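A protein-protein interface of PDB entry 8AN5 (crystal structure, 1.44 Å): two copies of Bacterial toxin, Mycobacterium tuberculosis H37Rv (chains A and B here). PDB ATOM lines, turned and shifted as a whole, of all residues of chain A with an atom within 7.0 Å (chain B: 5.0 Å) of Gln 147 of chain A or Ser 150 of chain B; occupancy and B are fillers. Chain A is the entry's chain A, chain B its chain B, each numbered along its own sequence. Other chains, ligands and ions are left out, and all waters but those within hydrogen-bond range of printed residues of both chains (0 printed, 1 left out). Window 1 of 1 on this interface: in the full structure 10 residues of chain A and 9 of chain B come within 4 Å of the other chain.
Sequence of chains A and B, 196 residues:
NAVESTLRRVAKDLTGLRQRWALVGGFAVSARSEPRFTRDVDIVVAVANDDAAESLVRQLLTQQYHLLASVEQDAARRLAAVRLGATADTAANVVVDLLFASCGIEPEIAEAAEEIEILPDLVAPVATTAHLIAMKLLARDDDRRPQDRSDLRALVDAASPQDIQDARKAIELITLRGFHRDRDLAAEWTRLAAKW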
ATOM      1  N   ARG A  36      30.143  24.113  19.712  1.00  0.00           N
ATOM      2  CA  ARG A  36      30.609  22.783  19.312  1.00  0.00           C
ATOM      3  C   ARG A  36      30.929  22.944  17.833  1.00  0.00           C
ATOM      4  O   ARG A  36      30.019  23.249  17.049  1.00  0.00           O
ATOM      5  CB  ARG A  36      29.498  21.766  19.485  1.00  0.00           C
ATOM      6  CG  ARG A  36      29.943  20.311  19.616  1.00  0.00           C
ATOM      7  CD  ARG A  36      30.478  19.667  18.324  1.00  0.00           C
ATOM      8  NE  ARG A  36      29.660  19.914  17.127  1.00  0.00           N
ATOM      9  CZ  ARG A  36      30.145  19.947  15.886  1.00  0.00           C
ATOM     10  NH1 ARG A  36      31.434  19.735  15.659  1.00  0.00           N
ATOM     11  NH2 ARG A  36      29.343  20.183  14.868  1.00  0.00           N
ATOM     12  N   THR A  38      34.327  22.216  14.596  1.00  0.00           N
ATOM     13  CA  THR A  38      35.617  21.715  14.128  1.00  0.00           C
ATOM     14  C   THR A  38      36.192  22.721  13.136  1.00  0.00           C
ATOM     15  O   THR A  38      35.740  23.869  13.084  1.00  0.00           O
ATOM     16  CB  THR A  38      35.449  20.319  13.513  1.00  0.00           C
ATOM     17  OG1 THR A  38      34.480  20.369  12.460  1.00  0.00           O
ATOM     18  CG2 THR A  38      35.045  19.299  14.575  1.00  0.00           C
ATOM     19  N   ASP A  40      35.919  22.844   9.980  1.00  0.00           N
ATOM     20  CA  ASP A  40      35.055  23.029   8.824  1.00  0.00           C
ATOM     21  C   ASP A  40      34.034  24.135   9.121  1.00  0.00           C
ATOM     22  O   ASP A  40      33.171  24.003   9.995  1.00  0.00           O
ATOM     23  CB  ASP A  40      34.303  21.728   8.513  1.00  0.00           C
ATOM     24  CG  ASP A  40      35.217  20.533   8.246  1.00  0.00           C
ATOM     25  OD1 ASP A  40      36.430  20.721   8.058  1.00  0.00           O
ATOM     26  OD2 ASP A  40      34.705  19.396   8.231  1.00  0.00           O
ATOM     27  N   LYS A 136      20.754  18.120  10.047  1.00  0.00           N
ATOM     28  CA  LYS A 136      21.475  17.184  10.925  1.00  0.00           C
ATOM     29  C   LYS A 136      20.797  15.818  10.887  1.00  0.00           C
ATOM     30  O   LYS A 136      21.486  14.870  10.856  1.00  0.00           O
ATOM     31  CB  LYS A 136      21.601  17.799  12.308  1.00  0.00           C
ATOM     32  CG  LYS A 136      22.644  18.911  12.357  1.00  0.00           C
ATOM     33  CD  LYS A 136      24.038  18.401  12.546  1.00  0.00           C
ATOM     34  CE  LYS A 136      25.058  19.510  12.453  1.00  0.00           C
ATOM     35  NZ  LYS A 136      26.423  18.981  12.638  1.00  0.00           N
ATOM     36  N   ASP A 141      25.148  10.274  10.727  1.00  0.00           N
ATOM     37  CA  ASP A 141      25.848   9.006  10.502  1.00  0.00           C
ATOM     38  C   ASP A 141      26.516   8.733  11.846  1.00  0.00           C
ATOM     39  O   ASP A 141      27.574   9.301  12.133  1.00  0.00           O
ATOM     40  CB  ASP A 141      26.868   9.130   9.374  1.00  0.00           C
ATOM     41  CG  ASP A 141      27.515   7.795   9.004  1.00  0.00           C
ATOM     42  OD1 ASP A 141      27.803   6.997   9.925  1.00  0.00           O
ATOM     43  OD2 ASP A 141      27.755   7.552   7.802  1.00  0.00           O
ATOM     44  N   ASP A 142      25.856   7.928  12.684  1.00  0.00           N
ATOM     45  CA  ASP A 142      26.336   7.704  14.044  1.00  0.00           C
ATOM     46  C   ASP A 142      27.706   7.036  14.051  1.00  0.00           C
ATOM     47  O   ASP A 142      28.465   7.189  15.015  1.00  0.00           O
ATOM     48  CB  ASP A 142      25.320   6.850  14.802  1.00  0.00           C
ATOM     49  CG  ASP A 142      24.130   7.651  15.287  1.00  0.00           C
ATOM     50  OD1 ASP A 142      23.979   8.812  14.847  1.00  0.00           O
ATOM     51  OD2 ASP A 142      23.344   7.118  16.102  1.00  0.00           O
ATOM     52  N   ARG A 144      30.324   7.442  11.546  1.00  0.00           N
ATOM     53  CA  ARG A 144      31.396   8.326  11.101  1.00  0.00           C
ATOM     54  C   ARG A 144      31.236   9.772  11.560  1.00  0.00           C
ATOM     55  O   ARG A 144      32.227  10.513  11.559  1.00  0.00           O
ATOM     56  CB  ARG A 144      31.467   8.311   9.569  1.00  0.00           C
ATOM     57  CG  ARG A 144      31.584   6.920   8.954  1.00  0.00           C
ATOM     58  CD  ARG A 144      32.996   6.367   9.043  1.00  0.00           C
ATOM     59  NE  ARG A 144      33.054   4.944   8.710  1.00  0.00           N
ATOM     60  CZ  ARG A 144      33.473   4.449   7.547  1.00  0.00           C
ATOM     61  NH1 ARG A 144      33.866   5.256   6.571  1.00  0.00           N
ATOM     62  NH2 ARG A 144      33.488   3.139   7.357  1.00  0.00           N
ATOM     63  N   ARG A 145      30.027  10.198  11.932  1.00  0.00           N
ATOM     64  CA  ARG A 145      29.770  11.574  12.367  1.00  0.00           C
ATOM     65  C   ARG A 145      28.887  11.578  13.611  1.00  0.00           C
ATOM     66  O   ARG A 145      27.701  11.922  13.550  1.00  0.00           O
ATOM     67  CB  ARG A 145      29.110  12.387  11.251  1.00  0.00           C
ATOM     68  CG  ARG A 145      29.710  12.235   9.865  1.00  0.00           C
ATOM     69  CD  ARG A 145      29.113  13.286   8.924  1.00  0.00           C
ATOM     70  NE  ARG A 145      29.797  14.572   9.029  1.00  0.00           N
ATOM     71  CZ  ARG A 145      29.227  15.753   8.800  1.00  0.00           C
ATOM     72  NH1 ARG A 145      27.951  15.829   8.440  1.00  0.00           N
ATOM     73  NH2 ARG A 145      29.937  16.866   8.929  1.00  0.00           N
ATOM     74  N   PRO A 146      29.438  11.200  14.767  1.00  0.00           N
ATOM     75  CA  PRO A 146      28.633  11.260  16.002  1.00  0.00           C
ATOM     76  C   PRO A 146      28.276  12.674  16.457  1.00  0.00           C
ATOM     77  O   PRO A 146      27.349  12.821  17.264  1.00  0.00           O
ATOM     78  CB  PRO A 146      29.496  10.537  17.045  1.00  0.00           C
ATOM     79  CG  PRO A 146      30.513   9.774  16.289  1.00  0.00           C
ATOM     80  CD  PRO A 146      30.615  10.325  14.894  1.00  0.00           C
ATOM     81  N   GLN A 147      28.968  13.714  15.979  1.00  0.00           N
ATOM     82  CA  GLN A 147      28.630  15.077  16.387  1.00  0.00           C
ATOM     83  C   GLN A 147      27.247  15.506  15.900  1.00  0.00           C
ATOM     84  O   GLN A 147      26.650  16.418  16.481  1.00  0.00           O
ATOM     85  CB  GLN A 147      29.682  16.077  15.882  1.00  0.00           C
ATOM     86  CG  GLN A 147      29.596  16.425  14.390  1.00  0.00           C
ATOM     87  CD  GLN A 147      30.470  15.540  13.516  1.00  0.00           C
ATOM     88  OE1 GLN A 147      30.953  14.496  13.955  1.00  0.00           O
ATOM     89  NE2 GLN A 147      30.684  15.961  12.269  1.00  0.00           N
ATOM     90  N   ASP A 148      26.674  14.765  14.929  1.00  0.00           N
ATOM     91  CA  ASP A 148      25.419  15.142  14.231  1.00  0.00           C
ATOM     92  C   ASP A 148      24.261  14.842  15.166  1.00  0.00           C
ATOM     93  O   ASP A 148      23.311  15.645  15.251  1.00  0.00           O
ATOM     94  CB  ASP A 148      25.282  14.410  12.894  1.00  0.00           C
ATOM     95  CG  ASP A 148      26.020  15.083  11.751  1.00  0.00           C
ATOM     96  OD1 ASP A 148      26.455  16.238  11.936  1.00  0.00           O
ATOM     97  OD2 ASP A 148      26.156  14.449  10.687  1.00  0.00           O
ATOM     98  N   ARG A 149      24.380  13.702  15.831  1.00  0.00           N
ATOM     99  CA  ARG A 149      23.393  13.197  16.819  1.00  0.00           C
ATOM    100  C   ARG A 149      23.475  14.037  18.097  1.00  0.00           C
ATOM    101  O   ARG A 149      22.418  14.226  18.732  1.00  0.00           O
ATOM    102  CB  ARG A 149      23.650  11.717  17.121  1.00  0.00           C
ATOM    103  CG  ARG A 149      22.807  11.159  18.259  1.00  0.00           C
ATOM    104  CD  ARG A 149      22.905   9.649  18.365  1.00  0.00           C
ATOM    105  NE  ARG A 149      22.946   9.196  19.749  1.00  0.00           N
ATOM    106  CZ  ARG A 149      22.212   8.201  20.236  1.00  0.00           C
ATOM    107  NH1 ARG A 149      21.374   7.550  19.448  1.00  0.00           N
ATOM    108  NH2 ARG A 149      22.319   7.862  21.509  1.00  0.00           N
ATOM    109  N   SER A 150      24.667  14.524  18.471  1.00  0.00           N
ATOM    110  CA  SER A 150      24.836  15.330  19.700  1.00  0.00           C
ATOM    111  C   SER A 150      24.422  16.765  19.405  1.00  0.00           C
ATOM    112  O   SER A 150      23.731  17.334  20.194  1.00  0.00           O
ATOM    113  CB  SER A 150      26.204  15.166  20.232  1.00  0.00           C
ATOM    114  OG  SER A 150      27.148  15.758  19.411  1.00  0.00           O
ATOM    115  N   ASP A 151      24.777  17.269  18.237  1.00  0.00           N
ATOM    116  CA  ASP A 151      24.223  18.533  17.771  1.00  0.00           C
ATOM    117  C   ASP A 151      22.705  18.470  17.748  1.00  0.00           C
ATOM    118  O   ASP A 151      22.024  19.467  18.020  1.00  0.00           O
ATOM    119  CB  ASP A 151      24.725  18.838  16.363  1.00  0.00           C
ATOM    120  CG  ASP A 151      26.085  19.467  16.357  1.00  0.00           C
ATOM    121  OD1 ASP A 151      26.697  19.561  17.432  1.00  0.00           O
ATOM    122  OD2 ASP A 151      26.539  19.878  15.275  1.00  0.00           O
ATOM    123  N   LEU A 152      22.137  17.312  17.430  1.00  0.00           N
ATOM    124  CA  LEU A 152      20.664  17.165  17.306  1.00  0.00           C
ATOM    125  C   LEU A 152      19.974  17.343  18.650  1.00  0.00           C
ATOM    126  O   LEU A 152      19.036  18.038  18.728  1.00  0.00           O
ATOM    127  CB  LEU A 152      20.342  15.793  16.716  1.00  0.00           C
ATOM    128  CG  LEU A 152      18.988  15.670  16.026  1.00  0.00           C
ATOM    129  CD1 LEU A 152      18.720  16.819  15.072  1.00  0.00           C
ATOM    130  CD2 LEU A 152      18.909  14.359  15.263  1.00  0.00           C
ATOM    131  N   ARG A 153      20.503  16.688  19.683  1.00  0.00           N
ATOM    132  CA  ARG A 153      19.958  16.776  21.056  1.00  0.00           C
ATOM    133  C   ARG A 153      19.939  18.256  21.440  1.00  0.00           C
ATOM    134  O   ARG A 153      18.878  18.735  21.853  1.00  0.00           O
ATOM    135  CB  ARG A 153      20.801  15.944  22.027  1.00  0.00           C
ATOM    136  CG  ARG A 153      20.375  16.067  23.483  1.00  0.00           C
ATOM    137  CD  ARG A 153      18.917  15.702  23.690  1.00  0.00           C
ATOM    138  NE  ARG A 153      18.592  15.497  25.094  1.00  0.00           N
ATOM    139  CZ  ARG A 153      19.169  14.591  25.875  1.00  0.00           C
ATOM    140  NH1 ARG A 153      20.109  13.797  25.389  1.00  0.00           N
ATOM    141  NH2 ARG A 153      18.805  14.481  27.140  1.00  0.00           N
ATOM    142  N   PRO B 146      28.719  13.338  25.202  1.00  0.00           N
ATOM    143  CA  PRO B 146      28.627  12.802  23.834  1.00  0.00           C
ATOM    144  C   PRO B 146      29.861  13.074  22.996  1.00  0.00           C
ATOM    145  O   PRO B 146      30.091  12.376  21.999  1.00  0.00           O
ATOM    146  CB  PRO B 146      27.403  13.526  23.262  1.00  0.00           C
ATOM    147  CG  PRO B 146      27.444  14.869  23.944  1.00  0.00           C
ATOM    148  CD  PRO B 146      28.007  14.624  25.340  1.00  0.00           C
ATOM    149  N   GLN B 147      30.655  14.075  23.367  1.00  0.00           N
ATOM    150  CA  GLN B 147      31.854  14.414  22.617  1.00  0.00           C
ATOM    151  C   GLN B 147      32.895  13.304  22.655  1.00  0.00           C
ATOM    152  O   GLN B 147      33.835  13.319  21.852  1.00  0.00           O
ATOM    153  CB  GLN B 147      32.399  15.729  23.170  1.00  0.00           C
ATOM    154  CG  GLN B 147      33.400  16.437  22.284  1.00  0.00           C
ATOM    155  CD  GLN B 147      32.776  16.987  21.018  1.00  0.00           C
ATOM    156  OE1 GLN B 147      32.786  16.344  19.966  1.00  0.00           O
ATOM    157  NE2 GLN B 147      32.244  18.196  21.109  1.00  0.00           N
ATOM    158  N   ASP B 148      32.755  12.343  23.564  1.00  0.00           N
ATOM    159  CA  ASP B 148      33.717  11.248  23.613  1.00  0.00           C
ATOM    160  C   ASP B 148      33.611  10.369  22.372  1.00  0.00           C
ATOM    161  O   ASP B 148      34.634   9.932  21.828  1.00  0.00           O
ATOM    162  CB  ASP B 148      33.513  10.431  24.889  1.00  0.00           C
ATOM    163  CG  ASP B 148      33.910  11.203  26.142  1.00  0.00           C
ATOM    164  OD1 ASP B 148      34.841  12.028  26.060  1.00  0.00           O
ATOM    165  OD2 ASP B 148      33.299  10.981  27.208  1.00  0.00           O
ATOM    166  N   ARG B 149      32.385  10.115  21.900  1.00  0.00           N
ATOM    167  CA  ARG B 149      32.213   9.299  20.704  1.00  0.00           C
ATOM    168  C   ARG B 149      32.849   9.976  19.500  1.00  0.00           C
ATOM    169  O   ARG B 149      33.500   9.321  18.677  1.00  0.00           O
ATOM    170  CB  ARG B 149      30.725   9.028  20.458  1.00  0.00           C
ATOM    171  CG  ARG B 149      30.047   8.362  21.652  1.00  0.00           C
ATOM    172  CD  ARG B 149      28.581   7.937  21.442  1.00  0.00           C
ATOM    173  NE  ARG B 149      28.247   6.954  22.475  1.00  0.00           N
ATOM    174  CZ  ARG B 149      27.220   7.028  23.322  1.00  0.00           C
ATOM    175  NH1 ARG B 149      26.354   8.036  23.277  1.00  0.00           N
ATOM    176  NH2 ARG B 149      27.051   6.067  24.225  1.00  0.00           N
ATOM    177  N   SER B 150      32.680  11.297  19.390  1.00  0.00           N
ATOM    178  CA  SER B 150      33.263  12.027  18.274  1.00  0.00           C
ATOM    179  C   SER B 150      34.780  12.051  18.377  1.00  0.00           C
ATOM    180  O   SER B 150      35.477  11.882  17.369  1.00  0.00           O
ATOM    181  CB  SER B 150      32.711  13.451  18.261  1.00  0.00           C
ATOM    182  OG  SER B 150      31.310  13.418  18.060  1.00  0.00           O
ATOM    183  N   ASP B 151      35.312  12.285  19.583  1.00  0.00           N
ATOM    184  CA  ASP B 151      36.759  12.241  19.765  1.00  0.00           C
ATOM    185  C   ASP B 151      37.294  10.866  19.386  1.00  0.00           C
ATOM    186  O   ASP B 151      38.302  10.744  18.684  1.00  0.00           O
ATOM    187  CB  ASP B 151      37.093  12.545  21.220  1.00  0.00           C
ATOM    188  CG  ASP B 151      36.948  14.015  21.559  1.00  0.00           C
ATOM    189  OD1 ASP B 151      36.664  14.855  20.660  1.00  0.00           O
ATOM    190  OD2 ASP B 151      37.091  14.331  22.768  1.00  0.00           O
ATOM    191  N   LEU B 152      36.616   9.816  19.836  1.00  0.00           N
ATOM    192  CA  LEU B 152      37.070   8.468  19.532  1.00  0.00           C
ATOM    193  C   LEU B 152      37.098   8.218  18.027  1.00  0.00           C
ATOM    194  O   LEU B 152      38.062   7.632  17.513  1.00  0.00           O
ATOM    195  CB  LEU B 152      36.167   7.467  20.252  1.00  0.00           C
ATOM    196  CG  LEU B 152      36.459   5.979  20.129  1.00  0.00           C
ATOM    197  CD1 LEU B 152      37.862   5.621  20.535  1.00  0.00           C
ATOM    198  CD2 LEU B 152      35.454   5.194  20.977  1.00  0.00           C
ATOM    199  N   ARG B 153      36.071   8.643  17.310  1.00  0.00           N
ATOM    200  CA  ARG B 153      36.024   8.439  15.849  1.00  0.00           C
ATOM    201  C   ARG B 153      37.200   9.130  15.185  1.00  0.00           C
ATOM    202  O   ARG B 153      37.849   8.566  14.380  1.00  0.00           O
ATOM    203  CB  ARG B 153      34.710   8.971  15.279  1.00  0.00           C
ATOM    204  CG  ARG B 153      34.658   8.848  13.771  1.00  0.00           C
ATOM    205  CD  ARG B 153      35.050   7.446  13.378  1.00  0.00           C
ATOM    206  NE  ARG B 153      34.051   6.559  13.918  1.00  0.00           N
ATOM    207  CZ  ARG B 153      34.197   5.270  14.180  1.00  0.00           C
ATOM    208  NH1 ARG B 153      35.349   4.655  13.998  1.00  0.00           N
ATOM    209  NH2 ARG B 153      33.170   4.606  14.660  1.00  0.00           N
ATOM    210  N   ALA B 154      37.462  10.358  15.570  1.00  0.00           N
ATOM    211  CA  ALA B 154      38.579  11.117  15.031  1.00  0.00           C
ATOM    212  C   ALA B 154      39.901  10.431  15.324  1.00  0.00           C
ATOM    213  O   ALA B 154      40.769  10.343  14.449  1.00  0.00           O
ATOM    214  CB  ALA B 154      38.568  12.506  15.649  1.00  0.00           C
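OG of Ser 150 of chain B lies within hydrogen-bond range of N of Gln 147 of chain A, at 3.1 Å.
CG of Arg 36 of chain A touches NE2 of Gln 147 of chain B (3.5 Å).
Arg 144 of chain A touches Arg 153 of chain B.
Pro 146 of chain A touches Arg 149 of chain B.
Pro 146 of chain A touches Ser 150 of chain B.
Pro 146 of chain B touches Ser 150 of chain A.
Printed residues of chain A within 4 Å of Pro 146 of chain B: Ser 150.
Of the printed residues of chain A, Arg 149 of chain B touches Pro 146.
Ser 150 of chain B touches just these residues of chain A: Pro 146 (3.5 Å) and Gln 147 (3.1 Å).
Printed residues of chain A within 4 Å of Arg 153 of chain B: Arg 144 (3.7 Å).
The nearest printed residue of chain B that does not touch Gln 147 of chain A is Gln 147 of chain B (5.1 Å).
Pro 146 of chain A touches Arg 149 of chain B, but with the chains exchanged Arg 149 of chain A does not touch Pro 146 of chain B (6.5 Å).
Pro 146 of chain A touches Ser 150 of chain B, and with the chains exchanged Ser 150 of chain A touches Pro 146 of chain B.
Gln 147 of chain A touches Ser 150 of chain B, but with the chains exchanged Ser 150 of chain A does not touch Gln 147 of chain B (5.5 Å).
8 positions are printed for both chains.
Of the 6 pairs that touch across the chains among the printed residues, 2 have their exchanged pair printed and touching as well.
Of the 16 printed residues of chain A, 5 touch a printed residue of chain B.
Of the 9 printed residues of chain B, 5 touch a printed residue of chain A.
Among the printed residues, 6 pairs touch across the chains.
Among the printed residues, no Asp or Glu carboxylate lies within 4 Å of a Lys or Arg side-chain nitrogen of the other chain.
The side-chain hydroxyl of Ser 150 of chain A lies within hydrogen-bond range of the backbone carbonyl oxygen of Gln 147 of chain A, 3.0 Å away.
NH2 of Arg 36 of chain A is in salt-bridge range of OD2 of Asp 151 of chain A (2.8 Å).
The backbone NH (N) of Arg 144 of chain A lies within hydrogen-bond range of the side-chain carboxylate (OD1) of Asp 141 of chain A (3.0 Å).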
